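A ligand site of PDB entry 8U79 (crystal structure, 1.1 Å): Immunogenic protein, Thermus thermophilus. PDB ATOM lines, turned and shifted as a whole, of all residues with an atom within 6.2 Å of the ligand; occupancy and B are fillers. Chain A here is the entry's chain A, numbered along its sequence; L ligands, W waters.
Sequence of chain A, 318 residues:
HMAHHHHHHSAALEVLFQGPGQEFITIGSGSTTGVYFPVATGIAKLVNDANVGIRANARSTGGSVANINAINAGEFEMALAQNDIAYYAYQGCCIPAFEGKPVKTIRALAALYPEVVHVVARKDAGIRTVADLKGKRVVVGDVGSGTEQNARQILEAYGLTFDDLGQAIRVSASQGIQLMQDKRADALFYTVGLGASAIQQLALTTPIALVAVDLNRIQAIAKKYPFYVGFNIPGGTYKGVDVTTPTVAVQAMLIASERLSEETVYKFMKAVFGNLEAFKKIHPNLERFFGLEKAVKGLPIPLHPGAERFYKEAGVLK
Gly 30 touches the ligand (CA to O2, 3.8 Å).
C of Gly 34 touches O3 of the ligand, at 3.9 Å.
Gly 62 touches the ligand (O to O4, 3.9 Å).
Gly 63 touches the ligand.
Ser 145 touches the ligand.
Tyr 190 touches the ligand (OH to O2, 3.6 Å).
CG2 of Val 192 touches O3 of the ligand (3.5 Å).
Hydrophobic or aromatic side chains that line the ligand: Val 35, Tyr 36 and Val 192.
15 residues have an atom within 4 Å of the ligand: Gly 30, Gly 34, Val 35, Tyr 36, Gly 62, Gly 63, Ser 64, Gln 82, Glu 115, Ser 145, Gly 146, Thr 147, Tyr 190, Thr 191 and Val 192.
The nearest printed residue that does not touch the ligand is Ser 31 (4.2 Å).
OH of Tyr 36 lies within hydrogen-bond range of OG of Ser 64, at 3.4 Å.
The side-chain hydroxyl (OH) of Tyr 36 lies within hydrogen-bond range of the backbone NH (N) of Gln 82.
OH of Tyr 36 sits at hydrogen-bond distance from OE1 of Glu 115.
The backbone NH (N) of Thr 191 lies within hydrogen-bond range of the side-chain hydroxyl (OG1) of Thr 147.
The backbone NH of Ser 145 lies close to the backbone carbonyl oxygen of Gly 62, at 3.4 Å.
The side-chain hydroxyl (OG) of Ser 145 is in hydrogen-bond range of the backbone NH (N) of Glu 148 (3.0 Å).
The side-chain hydroxyl (OG) of Ser 145 sits at hydrogen-bond distance from the backbone carbonyl oxygen (O) of Asp 142 (2.7 Å).
The side-chain amide oxygen (OD1) of Asn 67 lies close to the backbone carbonyl oxygen (O) of Gly 63 (3.3 Å).
Water W3 lies within hydrogen-bond range of O2 of the ligand (2.6 Å), OH of Tyr 190 (2.7 Å) and N of Ser 31 (2.8 Å).
Water W2 lies within hydrogen-bond range of OE2 of Glu 115 (2.7 Å), OH of Tyr 113 (2.7 Å), O3 of the ligand (2.8 Å) and N of Gly 193 (3.0 Å).
Water W4 bridges an oxygen (O4) of the ligand (2.8 Å) and the backbone carbonyl oxygen (O) of Gly 62 (2.9 Å).
O1 of the ligand sits at hydrogen-bond distance from N of Ser 64, at 2.9 Å.
An oxygen (O1) of the ligand sits at hydrogen-bond distance from the side-chain hydroxyl of Ser 64 (2.7 Å).
A nitrogen (N1) of the ligand is in hydrogen-bond range of the side-chain amide oxygen (OE1) of Gln 82, at 2.7 Å.
OE2 of Glu 115 is in salt-bridge range of N1 of the ligand (2.8 Å).
The backbone NH (N) of Tyr 36 lies within hydrogen-bond range of an oxygen (O3) of the ligand (2.8 Å).
The side-chain hydroxyl (OH) of Tyr 36 sits at hydrogen-bond distance from a nitrogen (N1) of the ligand, 3.0 Å away.
N of Val 35 sits at hydrogen-bond distance from O3 of the ligand.
N of Gly 146 sits at hydrogen-bond distance from O4 of the ligand (3.0 Å).
O of Thr 191 sits close to N1 of the ligand, 3.2 Å away.
N of Thr 147 sits at hydrogen-bond distance from O4 of the ligand, at 3.4 Å.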
ATOM      1  N   SER A  29     -26.662   4.691 -19.775  1.00  0.00           N
ATOM      2  CA  SER A  29     -26.004   4.079 -20.912  1.00  0.00           C
ATOM      3  C   SER A  29     -25.208   5.123 -21.703  1.00  0.00           C
ATOM      4  O   SER A  29     -24.176   5.594 -21.235  1.00  0.00           O
ATOM      5  CB  SER A  29     -26.970   3.201 -21.698  1.00  0.00           C
ATOM      6  OG  SER A  29     -27.976   3.949 -22.375  1.00  0.00           O
ATOM      7  N   GLY A  30     -25.606   5.372 -22.941  1.00  0.00           N
ATOM      8  CA  GLY A  30     -24.897   6.286 -23.801  1.00  0.00           C
ATOM      9  C   GLY A  30     -25.815   6.692 -24.920  1.00  0.00           C
ATOM     10  O   GLY A  30     -27.019   6.623 -24.791  1.00  0.00           O
ATOM     11  N   SER A  31     -25.214   7.149 -26.025  1.00  0.00           N
ATOM     12  CA  SER A  31     -26.003   7.502 -27.209  1.00  0.00           C
ATOM     13  C   SER A  31     -26.774   6.287 -27.708  1.00  0.00           C
ATOM     14  O   SER A  31     -26.312   5.147 -27.626  1.00  0.00           O
ATOM     15  CB  SER A  31     -25.064   7.998 -28.309  1.00  0.00           C
ATOM     16  OG  SER A  31     -24.511   9.280 -28.046  1.00  0.00           O
ATOM     17  N   GLY A  34     -24.671   4.035 -29.918  1.00  0.00           N
ATOM     18  CA  GLY A  34     -23.475   3.389 -29.401  1.00  0.00           C
ATOM     19  C   GLY A  34     -23.769   1.944 -29.010  1.00  0.00           C
ATOM     20  O   GLY A  34     -24.731   1.334 -29.491  1.00  0.00           O
ATOM     21  N   VAL A  35     -22.915   1.372 -28.155  1.00  0.00           N
ATOM     22  CA  VAL A  35     -23.075   0.002 -27.713  1.00  0.00           C
ATOM     23  C   VAL A  35     -23.684  -0.077 -26.317  1.00  0.00           C
ATOM     24  O   VAL A  35     -24.474  -0.991 -26.008  1.00  0.00           O
ATOM     25  CB  VAL A  35     -21.732  -0.760 -27.832  1.00  0.00           C
ATOM     26  CG1 VAL A  35     -21.851  -2.185 -27.274  1.00  0.00           C
ATOM     27  CG2 VAL A  35     -21.298  -0.802 -29.288  1.00  0.00           C
ATOM     28  N   TYR A  36     -23.369   0.858 -25.411  1.00  0.00           N
ATOM     29  CA  TYR A  36     -23.979   0.842 -24.097  1.00  0.00           C
ATOM     30  C   TYR A  36     -25.504   0.796 -24.142  1.00  0.00           C
ATOM     31  O   TYR A  36     -26.118   0.078 -23.349  1.00  0.00           O
ATOM     32  CB  TYR A  36     -23.602   2.075 -23.284  1.00  0.00           C
ATOM     33  CG  TYR A  36     -22.190   2.207 -22.739  1.00  0.00           C
ATOM     34  CD1 TYR A  36     -21.230   1.225 -22.858  1.00  0.00           C
ATOM     35  CD2 TYR A  36     -21.880   3.358 -22.017  1.00  0.00           C
ATOM     36  CE1 TYR A  36     -19.963   1.392 -22.301  1.00  0.00           C
ATOM     37  CE2 TYR A  36     -20.635   3.527 -21.458  1.00  0.00           C
ATOM     38  CZ  TYR A  36     -19.661   2.561 -21.604  1.00  0.00           C
ATOM     39  OH  TYR A  36     -18.424   2.817 -21.081  1.00  0.00           O
ATOM     40  N   PHE A  37     -26.115   1.610 -25.026  1.00  0.00           N
ATOM     41  CA  PHE A  37     -27.561   1.704 -25.042  1.00  0.00           C
ATOM     42  C   PHE A  37     -28.212   0.364 -25.428  1.00  0.00           C
ATOM     43  O   PHE A  37     -29.084  -0.125 -24.693  1.00  0.00           O
ATOM     44  CB  PHE A  37     -28.024   2.868 -25.920  1.00  0.00           C
ATOM     45  CG  PHE A  37     -29.517   2.983 -25.935  1.00  0.00           C
ATOM     46  CD1 PHE A  37     -30.206   3.599 -24.905  1.00  0.00           C
ATOM     47  CD2 PHE A  37     -30.254   2.479 -26.996  1.00  0.00           C
ATOM     48  CE1 PHE A  37     -31.577   3.718 -24.923  1.00  0.00           C
ATOM     49  CE2 PHE A  37     -31.633   2.607 -27.021  1.00  0.00           C
ATOM     50  CZ  PHE A  37     -32.286   3.219 -25.982  1.00  0.00           C
ATOM     51  N   GLY A  62     -25.052  10.946 -21.871  1.00  0.00           N
ATOM     52  CA  GLY A  62     -23.784  11.351 -22.419  1.00  0.00           C
ATOM     53  C   GLY A  62     -22.656  10.336 -22.296  1.00  0.00           C
ATOM     54  O   GLY A  62     -21.595  10.525 -22.904  1.00  0.00           O
ATOM     55  N   GLY A  63     -22.853   9.317 -21.453  1.00  0.00           N
ATOM     56  CA  GLY A  63     -21.833   8.320 -21.249  1.00  0.00           C
ATOM     57  C   GLY A  63     -21.295   8.268 -19.824  1.00  0.00           C
ATOM     58  O   GLY A  63     -21.984   8.639 -18.865  1.00  0.00           O
ATOM     59  N   SER A  64     -20.027   7.829 -19.687  1.00  0.00           N
ATOM     60  CA  SER A  64     -19.520   7.380 -18.415  1.00  0.00           C
ATOM     61  C   SER A  64     -19.573   8.411 -17.292  1.00  0.00           C
ATOM     62  O   SER A  64     -19.902   8.069 -16.156  1.00  0.00           O
ATOM     63  CB  SER A  64     -18.105   6.914 -18.519  1.00  0.00           C
ATOM     64  OG  SER A  64     -17.937   5.728 -19.300  1.00  0.00           O
ATOM     65  N   VAL A  65     -19.113   9.636 -17.550  1.00  0.00           N
ATOM     66  CA  VAL A  65     -19.078  10.634 -16.469  1.00  0.00           C
ATOM     67  C   VAL A  65     -20.491  11.000 -16.025  1.00  0.00           C
ATOM     68  O   VAL A  65     -20.797  11.008 -14.823  1.00  0.00           O
ATOM     69  CB  VAL A  65     -18.276  11.893 -16.925  1.00  0.00           C
ATOM     70  CG1 VAL A  65     -18.397  12.997 -15.886  1.00  0.00           C
ATOM     71  CG2 VAL A  65     -16.821  11.561 -17.189  1.00  0.00           C
ATOM     72  N   ASN A  67     -23.067   9.167 -16.242  1.00  0.00           N
ATOM     73  CA  ASN A  67     -23.653   8.006 -15.594  1.00  0.00           C
ATOM     74  C   ASN A  67     -23.204   7.888 -14.140  1.00  0.00           C
ATOM     75  O   ASN A  67     -24.026   7.593 -13.271  1.00  0.00           O
ATOM     76  CB  ASN A  67     -23.269   6.735 -16.335  1.00  0.00           C
ATOM     77  CG  ASN A  67     -23.949   6.612 -17.694  1.00  0.00           C
ATOM     78  OD1 ASN A  67     -24.913   7.337 -17.973  1.00  0.00           O
ATOM     79  ND2 ASN A  67     -23.461   5.667 -18.484  1.00  0.00           N
ATOM     80  N   LEU A  80     -23.628   1.629 -17.358  1.00  0.00           N
ATOM     81  CA  LEU A  80     -22.404   1.252 -18.032  1.00  0.00           C
ATOM     82  C   LEU A  80     -21.370   2.375 -17.820  1.00  0.00           C
ATOM     83  O   LEU A  80     -21.701   3.558 -17.799  1.00  0.00           O
ATOM     84  CB  LEU A  80     -22.647   1.066 -19.527  1.00  0.00           C
ATOM     85  CG  LEU A  80     -23.419  -0.162 -19.967  1.00  0.00           C
ATOM     86  CD1 LEU A  80     -22.561  -1.360 -19.785  1.00  0.00           C
ATOM     87  CD2 LEU A  80     -24.670  -0.510 -19.248  1.00  0.00           C
ATOM     88  N   ALA A  81     -20.091   2.006 -17.739  1.00  0.00           N
ATOM     89  CA  ALA A  81     -19.032   2.998 -17.657  1.00  0.00           C
ATOM     90  C   ALA A  81     -17.704   2.339 -18.015  1.00  0.00           C
ATOM     91  O   ALA A  81     -17.504   1.142 -17.816  1.00  0.00           O
ATOM     92  CB  ALA A  81     -18.964   3.593 -16.259  1.00  0.00           C
ATOM     93  N   GLN A  82     -16.766   3.154 -18.466  1.00  0.00           N
ATOM     94  CA  GLN A  82     -15.423   2.689 -18.722  1.00  0.00           C
ATOM     95  C   GLN A  82     -14.681   2.434 -17.412  1.00  0.00           C
ATOM     96  O   GLN A  82     -14.851   3.137 -16.429  1.00  0.00           O
ATOM     97  CB  GLN A  82     -14.640   3.726 -19.504  1.00  0.00           C
ATOM     98  CG  GLN A  82     -15.202   4.067 -20.858  1.00  0.00           C
ATOM     99  CD  GLN A  82     -14.592   5.244 -21.610  1.00  0.00           C
ATOM    100  OE1 GLN A  82     -15.189   5.705 -22.584  1.00  0.00           O
ATOM    101  NE2 GLN A  82     -13.397   5.684 -21.253  1.00  0.00           N
ATOM    102  N   ILE A  85     -12.600   5.574 -16.233  1.00  0.00           N
ATOM    103  CA  ILE A  85     -13.428   6.609 -15.651  1.00  0.00           C
ATOM    104  C   ILE A  85     -13.943   6.164 -14.267  1.00  0.00           C
ATOM    105  O   ILE A  85     -13.981   6.978 -13.337  1.00  0.00           O
ATOM    106  CB  ILE A  85     -14.563   7.014 -16.585  1.00  0.00           C
ATOM    107  CG1 ILE A  85     -14.078   7.360 -17.992  1.00  0.00           C
ATOM    108  CG2 ILE A  85     -15.339   8.183 -15.975  1.00  0.00           C
ATOM    109  CD1 ILE A  85     -12.976   8.394 -18.079  1.00  0.00           C
ATOM    110  N   TYR A 113     -16.584  -5.976 -22.097  1.00  0.00           N
ATOM    111  CA  TYR A 113     -15.975  -6.099 -23.422  1.00  0.00           C
ATOM    112  C   TYR A 113     -15.046  -4.893 -23.609  1.00  0.00           C
ATOM    113  O   TYR A 113     -15.180  -3.894 -22.908  1.00  0.00           O
ATOM    114  CB  TYR A 113     -17.054  -6.128 -24.542  1.00  0.00           C
ATOM    115  CG  TYR A 113     -17.937  -4.910 -24.579  1.00  0.00           C
ATOM    116  CD1 TYR A 113     -17.540  -3.761 -25.303  1.00  0.00           C
ATOM    117  CD2 TYR A 113     -19.155  -4.882 -23.961  1.00  0.00           C
ATOM    118  CE1 TYR A 113     -18.305  -2.613 -25.257  1.00  0.00           C
ATOM    119  CE2 TYR A 113     -19.935  -3.737 -23.916  1.00  0.00           C
ATOM    120  CZ  TYR A 113     -19.505  -2.584 -24.583  1.00  0.00           C
ATOM    121  OH  TYR A 113     -20.245  -1.431 -24.503  1.00  0.00           O
ATOM    122  N   GLU A 115     -13.610  -1.462 -25.110  1.00  0.00           N
ATOM    123  CA  GLU A 115     -14.053  -0.241 -25.764  1.00  0.00           C
ATOM    124  C   GLU A 115     -12.867   0.400 -26.441  1.00  0.00           C
ATOM    125  O   GLU A 115     -11.862   0.707 -25.795  1.00  0.00           O
ATOM    126  CB  GLU A 115     -14.709   0.746 -24.825  1.00  0.00           C
ATOM    127  CG  GLU A 115     -15.860   0.161 -24.034  1.00  0.00           C
ATOM    128  CD  GLU A 115     -16.659   1.254 -23.393  1.00  0.00           C
ATOM    129  OE1 GLU A 115     -16.576   1.362 -22.138  1.00  0.00           O
ATOM    130  OE2 GLU A 115     -17.373   1.966 -24.143  1.00  0.00           O
ATOM    131  N   ASP A 142     -19.289  13.239 -26.367  1.00  0.00           N
ATOM    132  CA  ASP A 142     -20.455  13.915 -25.842  1.00  0.00           C
ATOM    133  C   ASP A 142     -20.128  14.604 -24.521  1.00  0.00           C
ATOM    134  O   ASP A 142     -19.128  14.332 -23.839  1.00  0.00           O
ATOM    135  CB  ASP A 142     -21.605  12.925 -25.686  1.00  0.00           C
ATOM    136  CG  ASP A 142     -22.998  13.502 -25.752  1.00  0.00           C
ATOM    137  OD1 ASP A 142     -23.126  14.763 -25.769  1.00  0.00           O
ATOM    138  OD2 ASP A 142     -23.940  12.683 -25.790  1.00  0.00           O
ATOM    139  N   GLY A 144     -20.283  14.870 -20.821  1.00  0.00           N
ATOM    140  CA  GLY A 144     -20.358  13.820 -19.843  1.00  0.00           C
ATOM    141  C   GLY A 144     -19.877  12.461 -20.309  1.00  0.00           C
ATOM    142  O   GLY A 144     -20.129  11.438 -19.665  1.00  0.00           O
ATOM    143  N   SER A 145     -19.142  12.412 -21.416  1.00  0.00           N
ATOM    144  CA  SER A 145     -18.646  11.180 -21.955  1.00  0.00           C
ATOM    145  C   SER A 145     -17.299  10.780 -21.382  1.00  0.00           C
ATOM    146  O   SER A 145     -16.444  11.590 -21.001  1.00  0.00           O
ATOM    147  CB  SER A 145     -18.514  11.260 -23.484  1.00  0.00           C
ATOM    148  OG  SER A 145     -17.512  12.183 -23.898  1.00  0.00           O
ATOM    149  N   GLY A 146     -17.065   9.455 -21.368  1.00  0.00           N
ATOM    150  CA  GLY A 146     -15.716   8.911 -21.273  1.00  0.00           C
ATOM    151  C   GLY A 146     -14.855   9.310 -22.472  1.00  0.00           C
ATOM    152  O   GLY A 146     -13.666   9.614 -22.334  1.00  0.00           O
ATOM    153  N   THR A 147     -15.480   9.301 -23.646  1.00  0.00           N
ATOM    154  CA  THR A 147     -14.783   9.599 -24.908  1.00  0.00           C
ATOM    155  C   THR A 147     -13.986  10.892 -24.805  1.00  0.00           C
ATOM    156  O   THR A 147     -12.810  10.918 -25.208  1.00  0.00           O
ATOM    157  CB  THR A 147     -15.783   9.726 -26.034  1.00  0.00           C
ATOM    158  OG1 THR A 147     -16.482   8.499 -26.210  1.00  0.00           O
ATOM    159  CG2 THR A 147     -15.126  10.160 -27.330  1.00  0.00           C
ATOM    160  N   GLU A 148     -14.592  11.950 -24.288  1.00  0.00           N
ATOM    161  CA  GLU A 148     -13.905  13.234 -24.250  1.00  0.00           C
ATOM    162  C   GLU A 148     -12.635  13.162 -23.397  1.00  0.00           C
ATOM    163  O   GLU A 148     -11.661  13.864 -23.682  1.00  0.00           O
ATOM    164  CB  GLU A 148     -14.823  14.300 -23.706  1.00  0.00           C
ATOM    165  CG  GLU A 148     -14.208  15.655 -23.532  1.00  0.00           C
ATOM    166  CD  GLU A 148     -15.017  16.724 -22.880  1.00  0.00           C
ATOM    167  OE1 GLU A 148     -16.211  16.472 -22.682  1.00  0.00           O
ATOM    168  OE2 GLU A 148     -14.483  17.843 -22.604  1.00  0.00           O
ATOM    169  N   TYR A 190     -14.636   8.410 -30.673  1.00  0.00           N
ATOM    170  CA  TYR A 190     -15.641   7.643 -29.953  1.00  0.00           C
ATOM    171  C   TYR A 190     -14.926   6.497 -29.265  1.00  0.00           C
ATOM    172  O   TYR A 190     -14.301   5.672 -29.926  1.00  0.00           O
ATOM    173  CB  TYR A 190     -16.742   7.129 -30.892  1.00  0.00           C
ATOM    174  CG  TYR A 190     -18.086   6.796 -30.262  1.00  0.00           C
ATOM    175  CD1 TYR A 190     -18.396   7.016 -28.937  1.00  0.00           C
ATOM    176  CD2 TYR A 190     -19.105   6.309 -31.070  1.00  0.00           C
ATOM    177  CE1 TYR A 190     -19.663   6.804 -28.441  1.00  0.00           C
ATOM    178  CE2 TYR A 190     -20.366   6.063 -30.568  1.00  0.00           C
ATOM    179  CZ  TYR A 190     -20.661   6.356 -29.254  1.00  0.00           C
ATOM    180  OH  TYR A 190     -21.949   6.155 -28.806  1.00  0.00           O
ATOM    181  N   THR A 191     -14.957   6.463 -27.917  1.00  0.00           N
ATOM    182  CA  THR A 191     -14.479   5.295 -27.174  1.00  0.00           C
ATOM    183  C   THR A 191     -15.671   4.342 -27.032  1.00  0.00           C
ATOM    184  O   THR A 191     -16.616   4.644 -26.328  1.00  0.00           O
ATOM    185  CB  THR A 191     -13.937   5.682 -25.794  1.00  0.00           C
ATOM    186  OG1 THR A 191     -12.904   6.651 -25.977  1.00  0.00           O
ATOM    187  CG2 THR A 191     -13.414   4.473 -25.061  1.00  0.00           C
ATOM    188  N   VAL A 192     -15.636   3.243 -27.821  1.00  0.00           N
ATOM    189  CA  VAL A 192     -16.858   2.446 -27.981  1.00  0.00           C
ATOM    190  C   VAL A 192     -16.486   1.044 -28.407  1.00  0.00           C
ATOM    191  O   VAL A 192     -15.472   0.816 -29.068  1.00  0.00           O
ATOM    192  CB  VAL A 192     -17.801   3.144 -29.005  1.00  0.00           C
ATOM    193  CG1 VAL A 192     -17.214   3.189 -30.405  1.00  0.00           C
ATOM    194  CG2 VAL A 192     -19.206   2.544 -29.009  1.00  0.00           C
ATOM    195  N   GLY A 193     -17.349   0.092 -28.069  1.00  0.00           N
ATOM    196  CA  GLY A 193     -17.173  -1.239 -28.597  1.00  0.00           C
ATOM    197  C   GLY A 193     -17.218  -1.256 -30.121  1.00  0.00           C
ATOM    198  O   GLY A 193     -17.860  -0.422 -30.761  1.00  0.00           O
HETATM  199  N1  LIG L   1     -17.583   4.630 -23.325  1.00  0.00           N
HETATM  200  C1  LIG L   1     -18.326   5.753 -23.945  1.00  0.00           C
HETATM  201  C2  LIG L   1     -18.430   6.902 -22.975  1.00  0.00           C
HETATM  202  O1  LIG L   1     -18.389   6.682 -21.774  1.00  0.00           O
HETATM  203  C3  LIG L   1     -19.703   5.350 -24.410  1.00  0.00           C
HETATM  204  C4  LIG L   1     -19.749   4.100 -25.289  1.00  0.00           C
HETATM  205  C5  LIG L   1     -21.111   3.650 -25.733  1.00  0.00           C
HETATM  206  O2  LIG L   1     -22.088   4.416 -25.605  1.00  0.00           O
HETATM  207  O3  LIG L   1     -21.187   2.483 -26.184  1.00  0.00           O
HETATM  208  O4  LIG L   1     -18.634   8.034 -23.437  1.00  0.00           O
HETATM  209  O   HOH W   1     -24.617   3.636 -26.222  1.00  0.00           O
HETATM  210  O   HOH W   2     -19.123   0.700 -25.788  1.00  0.00           O
HETATM  211  O   HOH W   3     -22.388   6.948 -26.241  1.00  0.00           O
HETATM  212  O   HOH W   4     -20.792   8.873 -25.085  1.00  0.00           O
